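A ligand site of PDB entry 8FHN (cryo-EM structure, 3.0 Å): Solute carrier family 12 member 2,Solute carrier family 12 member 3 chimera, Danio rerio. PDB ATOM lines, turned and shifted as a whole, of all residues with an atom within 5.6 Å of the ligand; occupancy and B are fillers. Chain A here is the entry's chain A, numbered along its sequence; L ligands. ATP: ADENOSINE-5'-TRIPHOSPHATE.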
ATOM      1  N   LEU A 719     -12.622   4.267 -14.398  1.00  0.00           N
ATOM      2  CA  LEU A 719     -13.781   4.705 -15.173  1.00  0.00           C
ATOM      3  C   LEU A 719     -14.200   6.085 -14.685  1.00  0.00           C
ATOM      4  O   LEU A 719     -15.083   6.238 -13.831  1.00  0.00           O
ATOM      5  CB  LEU A 719     -14.919   3.707 -15.050  1.00  0.00           C
ATOM      6  CG  LEU A 719     -14.771   2.388 -15.805  1.00  0.00           C
ATOM      7  CD1 LEU A 719     -16.049   1.612 -15.689  1.00  0.00           C
ATOM      8  CD2 LEU A 719     -14.449   2.659 -17.252  1.00  0.00           C
ATOM      9  N   THR A 720     -13.572   7.108 -15.251  1.00  0.00           N
ATOM     10  CA  THR A 720     -13.820   8.477 -14.824  1.00  0.00           C
ATOM     11  C   THR A 720     -14.919   9.177 -15.592  1.00  0.00           C
ATOM     12  O   THR A 720     -15.593  10.038 -15.036  1.00  0.00           O
ATOM     13  CB  THR A 720     -12.553   9.322 -14.967  1.00  0.00           C
ATOM     14  OG1 THR A 720     -12.124   9.308 -16.325  1.00  0.00           O
ATOM     15  CG2 THR A 720     -11.457   8.788 -14.104  1.00  0.00           C
ATOM     16  N   GLY A 721     -15.118   8.845 -16.864  1.00  0.00           N
ATOM     17  CA  GLY A 721     -15.802   9.746 -17.740  1.00  0.00           C
ATOM     18  C   GLY A 721     -14.856  10.886 -18.021  1.00  0.00           C
ATOM     19  O   GLY A 721     -13.637  10.728 -17.897  1.00  0.00           O
ATOM     20  N   PRO A 722     -15.372  12.048 -18.414  1.00  0.00           N
ATOM     21  CA  PRO A 722     -14.502  13.194 -18.621  1.00  0.00           C
ATOM     22  C   PRO A 722     -13.760  13.529 -17.334  1.00  0.00           C
ATOM     23  O   PRO A 722     -14.403  13.865 -16.324  1.00  0.00           O
ATOM     24  CB  PRO A 722     -15.471  14.318 -18.997  1.00  0.00           C
ATOM     25  CG  PRO A 722     -16.709  13.633 -19.412  1.00  0.00           C
ATOM     26  CD  PRO A 722     -16.785  12.377 -18.610  1.00  0.00           C
ATOM     27  N   ARG A 726     -15.101  13.898 -12.528  1.00  0.00           N
ATOM     28  CA  ARG A 726     -14.793  13.186 -11.296  1.00  0.00           C
ATOM     29  C   ARG A 726     -13.310  13.280 -10.978  1.00  0.00           C
ATOM     30  O   ARG A 726     -12.546  12.385 -11.318  1.00  0.00           O
ATOM     31  CB  ARG A 726     -15.221  11.730 -11.412  1.00  0.00           C
ATOM     32  CG  ARG A 726     -16.670  11.566 -11.831  1.00  0.00           C
ATOM     33  CD  ARG A 726     -17.008  10.141 -12.199  1.00  0.00           C
ATOM     34  NE  ARG A 726     -18.357  10.020 -12.725  1.00  0.00           N
ATOM     35  CZ  ARG A 726     -18.752  10.484 -13.894  1.00  0.00           C
ATOM     36  NH1 ARG A 726     -17.920  11.076 -14.723  1.00  0.00           N
ATOM     37  NH2 ARG A 726     -20.029  10.339 -14.265  1.00  0.00           N
ATOM     38  N   LEU A 729     -11.796  10.960  -7.961  1.00  0.00           N
ATOM     39  CA  LEU A 729     -11.551   9.576  -8.286  1.00  0.00           C
ATOM     40  C   LEU A 729     -10.306   9.401  -9.143  1.00  0.00           C
ATOM     41  O   LEU A 729      -9.813   8.279  -9.272  1.00  0.00           O
ATOM     42  CB  LEU A 729     -12.798   9.001  -8.982  1.00  0.00           C
ATOM     43  CG  LEU A 729     -13.029   7.519  -9.227  1.00  0.00           C
ATOM     44  CD1 LEU A 729     -14.500   7.262  -9.200  1.00  0.00           C
ATOM     45  CD2 LEU A 729     -12.546   7.172 -10.571  1.00  0.00           C
ATOM     46  N   GLY A 746     -10.551   5.863 -18.409  1.00  0.00           N
ATOM     47  CA  GLY A 746     -11.463   5.466 -19.459  1.00  0.00           C
ATOM     48  C   GLY A 746     -12.585   6.461 -19.676  1.00  0.00           C
ATOM     49  O   GLY A 746     -12.845   7.357 -18.884  1.00  0.00           O
ATOM     50  N   HIS A 747     -13.273   6.290 -20.802  1.00  0.00           N
ATOM     51  CA  HIS A 747     -14.363   7.173 -21.200  1.00  0.00           C
ATOM     52  C   HIS A 747     -15.163   6.528 -22.319  1.00  0.00           C
ATOM     53  O   HIS A 747     -14.585   6.076 -23.313  1.00  0.00           O
ATOM     54  CB  HIS A 747     -13.818   8.518 -21.646  1.00  0.00           C
ATOM     55  CG  HIS A 747     -14.867   9.569 -21.838  1.00  0.00           C
ATOM     56  ND1 HIS A 747     -14.571  10.864 -22.196  1.00  0.00           N
ATOM     57  CD2 HIS A 747     -16.221   9.519 -21.704  1.00  0.00           C
ATOM     58  CE1 HIS A 747     -15.685  11.573 -22.287  1.00  0.00           C
ATOM     59  NE2 HIS A 747     -16.697  10.777 -21.995  1.00  0.00           N
ATOM     60  N   VAL A 748     -16.480   6.483 -22.193  1.00  0.00           N
ATOM     61  CA  VAL A 748     -17.344   5.896 -23.197  1.00  0.00           C
ATOM     62  C   VAL A 748     -18.241   6.991 -23.740  1.00  0.00           C
ATOM     63  O   VAL A 748     -18.955   7.641 -22.977  1.00  0.00           O
ATOM     64  CB  VAL A 748     -18.168   4.739 -22.638  1.00  0.00           C
ATOM     65  CG1 VAL A 748     -19.163   4.270 -23.656  1.00  0.00           C
ATOM     66  CG2 VAL A 748     -17.272   3.603 -22.239  1.00  0.00           C
ATOM     67  N   LEU A 749     -18.186   7.204 -25.049  1.00  0.00           N
ATOM     68  CA  LEU A 749     -18.990   8.235 -25.709  1.00  0.00           C
ATOM     69  C   LEU A 749     -20.279   7.577 -26.170  1.00  0.00           C
ATOM     70  O   LEU A 749     -20.292   6.857 -27.165  1.00  0.00           O
ATOM     71  CB  LEU A 749     -18.233   8.858 -26.862  1.00  0.00           C
ATOM     72  CG  LEU A 749     -16.890   9.508 -26.530  1.00  0.00           C
ATOM     73  CD1 LEU A 749     -16.089   9.732 -27.769  1.00  0.00           C
ATOM     74  CD2 LEU A 749     -17.124  10.820 -25.835  1.00  0.00           C
ATOM     75  N   ILE A 750     -21.376   7.728 -25.455  1.00  0.00           N
ATOM     76  CA  ILE A 750     -22.575   6.989 -25.803  1.00  0.00           C
ATOM     77  C   ILE A 750     -23.386   7.667 -26.856  1.00  0.00           C
ATOM     78  O   ILE A 750     -24.079   8.626 -26.596  1.00  0.00           O
ATOM     79  CB  ILE A 750     -23.417   6.712 -24.555  1.00  0.00           C
ATOM     80  CG1 ILE A 750     -22.628   5.890 -23.547  1.00  0.00           C
ATOM     81  CG2 ILE A 750     -24.683   5.963 -24.921  1.00  0.00           C
ATOM     82  CD1 ILE A 750     -23.031   6.147 -22.117  1.00  0.00           C
ATOM     83  N   LEU A 788     -23.193   2.114 -21.879  1.00  0.00           N
ATOM     84  CA  LEU A 788     -21.971   2.196 -21.084  1.00  0.00           C
ATOM     85  C   LEU A 788     -21.361   0.824 -20.853  1.00  0.00           C
ATOM     86  O   LEU A 788     -20.148   0.696 -20.793  1.00  0.00           O
ATOM     87  CB  LEU A 788     -22.275   2.871 -19.747  1.00  0.00           C
ATOM     88  CG  LEU A 788     -21.106   3.391 -18.915  1.00  0.00           C
ATOM     89  CD1 LEU A 788     -21.631   4.489 -18.036  1.00  0.00           C
ATOM     90  CD2 LEU A 788     -20.459   2.339 -18.077  1.00  0.00           C
ATOM     91  N   VAL A 810     -11.513   0.238 -11.325  1.00  0.00           N
ATOM     92  CA  VAL A 810     -11.897   1.215 -10.314  1.00  0.00           C
ATOM     93  C   VAL A 810     -13.089   2.006 -10.848  1.00  0.00           C
ATOM     94  O   VAL A 810     -12.976   2.672 -11.874  1.00  0.00           O
ATOM     95  CB  VAL A 810     -10.743   2.152  -9.946  1.00  0.00           C
ATOM     96  CG1 VAL A 810     -11.147   3.086  -8.835  1.00  0.00           C
ATOM     97  CG2 VAL A 810      -9.534   1.349  -9.534  1.00  0.00           C
ATOM     98  N   VAL A 811     -14.208   1.923 -10.149  1.00  0.00           N
ATOM     99  CA  VAL A 811     -15.465   2.506 -10.626  1.00  0.00           C
ATOM    100  C   VAL A 811     -16.153   3.196  -9.450  1.00  0.00           C
ATOM    101  O   VAL A 811     -16.111   2.705  -8.328  1.00  0.00           O
ATOM    102  CB  VAL A 811     -16.365   1.424 -11.263  1.00  0.00           C
ATOM    103  CG1 VAL A 811     -16.624   0.305 -10.289  1.00  0.00           C
ATOM    104  CG2 VAL A 811     -17.661   2.019 -11.738  1.00  0.00           C
ATOM    105  N   GLY A 812     -16.761   4.340  -9.715  1.00  0.00           N
ATOM    106  CA  GLY A 812     -17.479   5.065  -8.698  1.00  0.00           C
ATOM    107  C   GLY A 812     -18.799   4.391  -8.363  1.00  0.00           C
ATOM    108  O   GLY A 812     -19.213   3.416  -8.991  1.00  0.00           O
ATOM    109  N   PHE A 813     -19.469   4.923  -7.354  1.00  0.00           N
ATOM    110  CA  PHE A 813     -20.708   4.356  -6.856  1.00  0.00           C
ATOM    111  C   PHE A 813     -21.894   5.115  -7.444  1.00  0.00           C
ATOM    112  O   PHE A 813     -21.862   6.342  -7.552  1.00  0.00           O
ATOM    113  CB  PHE A 813     -20.772   4.405  -5.339  1.00  0.00           C
ATOM    114  CG  PHE A 813     -21.981   3.746  -4.757  1.00  0.00           C
ATOM    115  CD1 PHE A 813     -22.034   2.387  -4.605  1.00  0.00           C
ATOM    116  CD2 PHE A 813     -23.073   4.499  -4.347  1.00  0.00           C
ATOM    117  CE1 PHE A 813     -23.153   1.774  -4.065  1.00  0.00           C
ATOM    118  CE2 PHE A 813     -24.177   3.893  -3.815  1.00  0.00           C
ATOM    119  CZ  PHE A 813     -24.221   2.533  -3.673  1.00  0.00           C
ATOM    120  N   LYS A 814     -22.935   4.369  -7.810  1.00  0.00           N
ATOM    121  CA  LYS A 814     -24.108   4.964  -8.450  1.00  0.00           C
ATOM    122  C   LYS A 814     -25.029   5.502  -7.364  1.00  0.00           C
ATOM    123  O   LYS A 814     -25.849   4.776  -6.812  1.00  0.00           O
ATOM    124  CB  LYS A 814     -24.805   3.920  -9.321  1.00  0.00           C
ATOM    125  CG  LYS A 814     -25.945   4.469 -10.149  1.00  0.00           C
ATOM    126  CD  LYS A 814     -26.487   3.431 -11.096  1.00  0.00           C
ATOM    127  CE  LYS A 814     -27.696   3.971 -11.823  1.00  0.00           C
ATOM    128  NZ  LYS A 814     -27.338   5.107 -12.690  1.00  0.00           N
ATOM    129  N   LYS A 815     -24.888   6.794  -7.067  1.00  0.00           N
ATOM    130  CA  LYS A 815     -25.598   7.377  -5.933  1.00  0.00           C
ATOM    131  C   LYS A 815     -27.107   7.366  -6.134  1.00  0.00           C
ATOM    132  O   LYS A 815     -27.861   7.130  -5.187  1.00  0.00           O
ATOM    133  CB  LYS A 815     -25.129   8.807  -5.696  1.00  0.00           C
ATOM    134  CG  LYS A 815     -25.594   9.390  -4.369  1.00  0.00           C
ATOM    135  CD  LYS A 815     -25.954  10.855  -4.489  1.00  0.00           C
ATOM    136  CE  LYS A 815     -24.726  11.738  -4.384  1.00  0.00           C
ATOM    137  NZ  LYS A 815     -25.082  13.110  -3.917  1.00  0.00           N
ATOM    138  N   ASN A 816     -27.571   7.608  -7.360  1.00  0.00           N
ATOM    139  CA  ASN A 816     -28.986   7.822  -7.643  1.00  0.00           C
ATOM    140  C   ASN A 816     -29.664   6.571  -8.195  1.00  0.00           C
ATOM    141  O   ASN A 816     -30.537   6.666  -9.056  1.00  0.00           O
ATOM    142  CB  ASN A 816     -29.152   9.007  -8.590  1.00  0.00           C
ATOM    143  CG  ASN A 816     -28.506   8.763  -9.951  1.00  0.00           C
ATOM    144  OD1 ASN A 816     -28.036   7.676 -10.249  1.00  0.00           O
ATOM    145  ND2 ASN A 816     -28.491   9.802 -10.774  1.00  0.00           N
ATOM    146  N   TYR A 828     -25.168  -1.451 -14.481  1.00  0.00           N
ATOM    147  CA  TYR A 828     -24.136  -1.176 -13.482  1.00  0.00           C
ATOM    148  C   TYR A 828     -23.634  -2.455 -12.845  1.00  0.00           C
ATOM    149  O   TYR A 828     -22.422  -2.639 -12.678  1.00  0.00           O
ATOM    150  CB  TYR A 828     -24.667  -0.224 -12.424  1.00  0.00           C
ATOM    151  CG  TYR A 828     -23.595   0.282 -11.495  1.00  0.00           C
ATOM    152  CD1 TYR A 828     -22.650   1.208 -11.933  1.00  0.00           C
ATOM    153  CD2 TYR A 828     -23.523  -0.153 -10.190  1.00  0.00           C
ATOM    154  CE1 TYR A 828     -21.675   1.674 -11.089  1.00  0.00           C
ATOM    155  CE2 TYR A 828     -22.540   0.308  -9.347  1.00  0.00           C
ATOM    156  CZ  TYR A 828     -21.627   1.220  -9.792  1.00  0.00           C
ATOM    157  OH  TYR A 828     -20.658   1.678  -8.951  1.00  0.00           O
ATOM    158  N   GLY A 850     -20.777  12.878  -3.081  1.00  0.00           N
ATOM    159  CA  GLY A 850     -20.837  12.481  -4.479  1.00  0.00           C
ATOM    160  C   GLY A 850     -19.488  12.568  -5.156  1.00  0.00           C
ATOM    161  O   GLY A 850     -18.549  13.144  -4.614  1.00  0.00           O
ATOM    162  N   LEU A 851     -19.383  11.990  -6.348  1.00  0.00           N
ATOM    163  CA  LEU A 851     -18.179  12.047  -7.150  1.00  0.00           C
ATOM    164  C   LEU A 851     -18.269  13.029  -8.310  1.00  0.00           C
ATOM    165  O   LEU A 851     -17.298  13.714  -8.604  1.00  0.00           O
ATOM    166  CB  LEU A 851     -17.825  10.654  -7.688  1.00  0.00           C
ATOM    167  CG  LEU A 851     -17.151   9.706  -6.713  1.00  0.00           C
ATOM    168  CD1 LEU A 851     -17.403   8.275  -7.112  1.00  0.00           C
ATOM    169  CD2 LEU A 851     -15.675   9.964  -6.718  1.00  0.00           C
ATOM    170  N   ASN A 852     -19.415  13.094  -8.970  1.00  0.00           N
ATOM    171  CA  ASN A 852     -19.593  13.996 -10.101  1.00  0.00           C
ATOM    172  C   ASN A 852     -19.655  15.444  -9.614  1.00  0.00           C
ATOM    173  O   ASN A 852     -20.549  15.807  -8.851  1.00  0.00           O
ATOM    174  CB  ASN A 852     -20.864  13.641 -10.863  1.00  0.00           C
ATOM    175  CG  ASN A 852     -20.969  14.348 -12.194  1.00  0.00           C
ATOM    176  OD1 ASN A 852     -20.285  15.333 -12.450  1.00  0.00           O
ATOM    177  ND2 ASN A 852     -21.830  13.842 -13.060  1.00  0.00           N
ATOM    178  N   LYS A 855     -22.429  18.301 -11.669  1.00  0.00           N
ATOM    179  CA  LYS A 855     -23.772  18.407 -11.132  1.00  0.00           C
ATOM    180  C   LYS A 855     -23.785  19.212  -9.839  1.00  0.00           C
ATOM    181  O   LYS A 855     -24.184  18.710  -8.784  1.00  0.00           O
ATOM    182  CB  LYS A 855     -24.368  17.018 -10.898  1.00  0.00           C
ATOM    183  CG  LYS A 855     -24.481  16.169 -12.161  1.00  0.00           C
ATOM    184  CD  LYS A 855     -24.953  14.765 -11.841  1.00  0.00           C
ATOM    185  CE  LYS A 855     -26.419  14.744 -11.445  1.00  0.00           C
ATOM    186  NZ  LYS A 855     -27.306  15.134 -12.568  1.00  0.00           N
HETATM  187  PG  ATP L   1     -22.689  11.048  -9.035  1.00  0.00           P
HETATM  188  O1G ATP L   1     -23.323  11.941 -10.062  1.00  0.00           O
HETATM  189  O2G ATP L   1     -21.516  11.649  -8.312  1.00  0.00           O
HETATM  190  O3G ATP L   1     -23.675  10.351  -8.136  1.00  0.00           O
HETATM  191  PB  ATP L   1     -22.698   9.531 -11.331  1.00  0.00           P
HETATM  192  O1B ATP L   1     -22.113  10.481 -12.355  1.00  0.00           O
HETATM  193  O2B ATP L   1     -24.196   9.427 -11.171  1.00  0.00           O
HETATM  194  O3B ATP L   1     -22.046   9.873  -9.916  1.00  0.00           O
HETATM  195  PA  ATP L   1     -23.162   7.077 -12.378  1.00  0.00           P
HETATM  196  O1A ATP L   1     -23.702   7.800 -13.573  1.00  0.00           O
HETATM  197  O2A ATP L   1     -24.093   6.496 -11.357  1.00  0.00           O
HETATM  198  O3A ATP L   1     -22.160   8.056 -11.625  1.00  0.00           O
HETATM  199  O5' ATP L   1     -22.171   5.911 -12.854  1.00  0.00           O
HETATM  200  C5' ATP L   1     -21.388   5.264 -11.866  1.00  0.00           C
HETATM  201  C4' ATP L   1     -19.931   5.335 -12.276  1.00  0.00           C
HETATM  202  O4' ATP L   1     -19.749   4.757 -13.561  1.00  0.00           O
HETATM  203  C3' ATP L   1     -19.429   6.737 -12.423  1.00  0.00           C
HETATM  204  O3' ATP L   1     -19.062   7.323 -11.175  1.00  0.00           O
HETATM  205  C2' ATP L   1     -18.238   6.516 -13.300  1.00  0.00           C
HETATM  206  O2' ATP L   1     -17.170   6.004 -12.537  1.00  0.00           O
HETATM  207  C1' ATP L   1     -18.715   5.451 -14.255  1.00  0.00           C
HETATM  208  N9  ATP L   1     -19.224   6.130 -15.454  1.00  0.00           N
HETATM  209  C8  ATP L   1     -20.410   6.728 -15.590  1.00  0.00           C
HETATM  210  N7  ATP L   1     -20.537   7.267 -16.815  1.00  0.00           N
HETATM  211  C5  ATP L   1     -19.408   7.017 -17.492  1.00  0.00           C
HETATM  212  C6  ATP L   1     -18.888   7.295 -18.841  1.00  0.00           C
HETATM  213  N6  ATP L   1     -19.610   7.981 -19.747  1.00  0.00           N
HETATM  214  N1  ATP L   1     -17.665   6.851 -19.137  1.00  0.00           N
HETATM  215  C2  ATP L   1     -16.928   6.179 -18.257  1.00  0.00           C
HETATM  216  N3  ATP L   1     -17.336   5.889 -17.026  1.00  0.00           N
HETATM  217  C4  ATP L   1     -18.548   6.269 -16.592  1.00  0.00           C
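N of Leu 719 sits at hydrogen-bond distance from O of Val 810 (3.0 Å).
The backbone NH of Gly 721 is in hydrogen-bond range of the backbone carbonyl oxygen of Gly 746.
NH1 of Arg 726 is in hydrogen-bond range of O of Thr 720 (2.6 Å).
Residues that only touch the ligand: Leu 788 (3.2 Å), Lys 815 (3.2 Å), Gly 721 (3.5 Å), Tyr 828 (3.7 Å), Lys 855 (3.7 Å), Gly 850 (3.9 Å), Val 811 (3.9 Å) and His 747 (3.9 Å).
Hydrophobic or aromatic side chains within 4 Å of the ligand: Leu 719, His 747, Leu 788, Val 811, Tyr 828 and Leu 851.
The nearest printed residue that does not touch the ligand is Phe 813 (4.3 Å).
The backbone NH of Asn 852 sits at hydrogen-bond distance from an oxygen (O2G) of the ligand (2.6 Å).
The side-chain amino group (NZ) of Lys 814 lies within salt-bridge range of an oxygen (O2A) of the ligand, 3.8 Å away.
The backbone carbonyl oxygen (O) of Leu 719 lies within hydrogen-bond range of an oxygen (O2') of the ligand, at 2.5 Å.
An oxygen (O2') of the ligand sits at hydrogen-bond distance from the backbone NH (N) of Gly 812, 3.3 Å away.
An oxygen (O2G) of the ligand lies within hydrogen-bond range of the backbone NH (N) of Leu 851 (2.9 Å).
The backbone carbonyl oxygen of Val 748 sits at hydrogen-bond distance from a nitrogen (N6) of the ligand (3.3 Å).
The backbone NH (N) of Val 748 lies within hydrogen-bond range of a nitrogen (N1) of the ligand (3.3 Å).
An oxygen (O1B) of the ligand is in hydrogen-bond range of the side-chain amide nitrogen of Asn 852 (3.4 Å).
NH2 of Arg 726 is in salt-bridge range of O1B of the ligand, 2.8 Å away.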
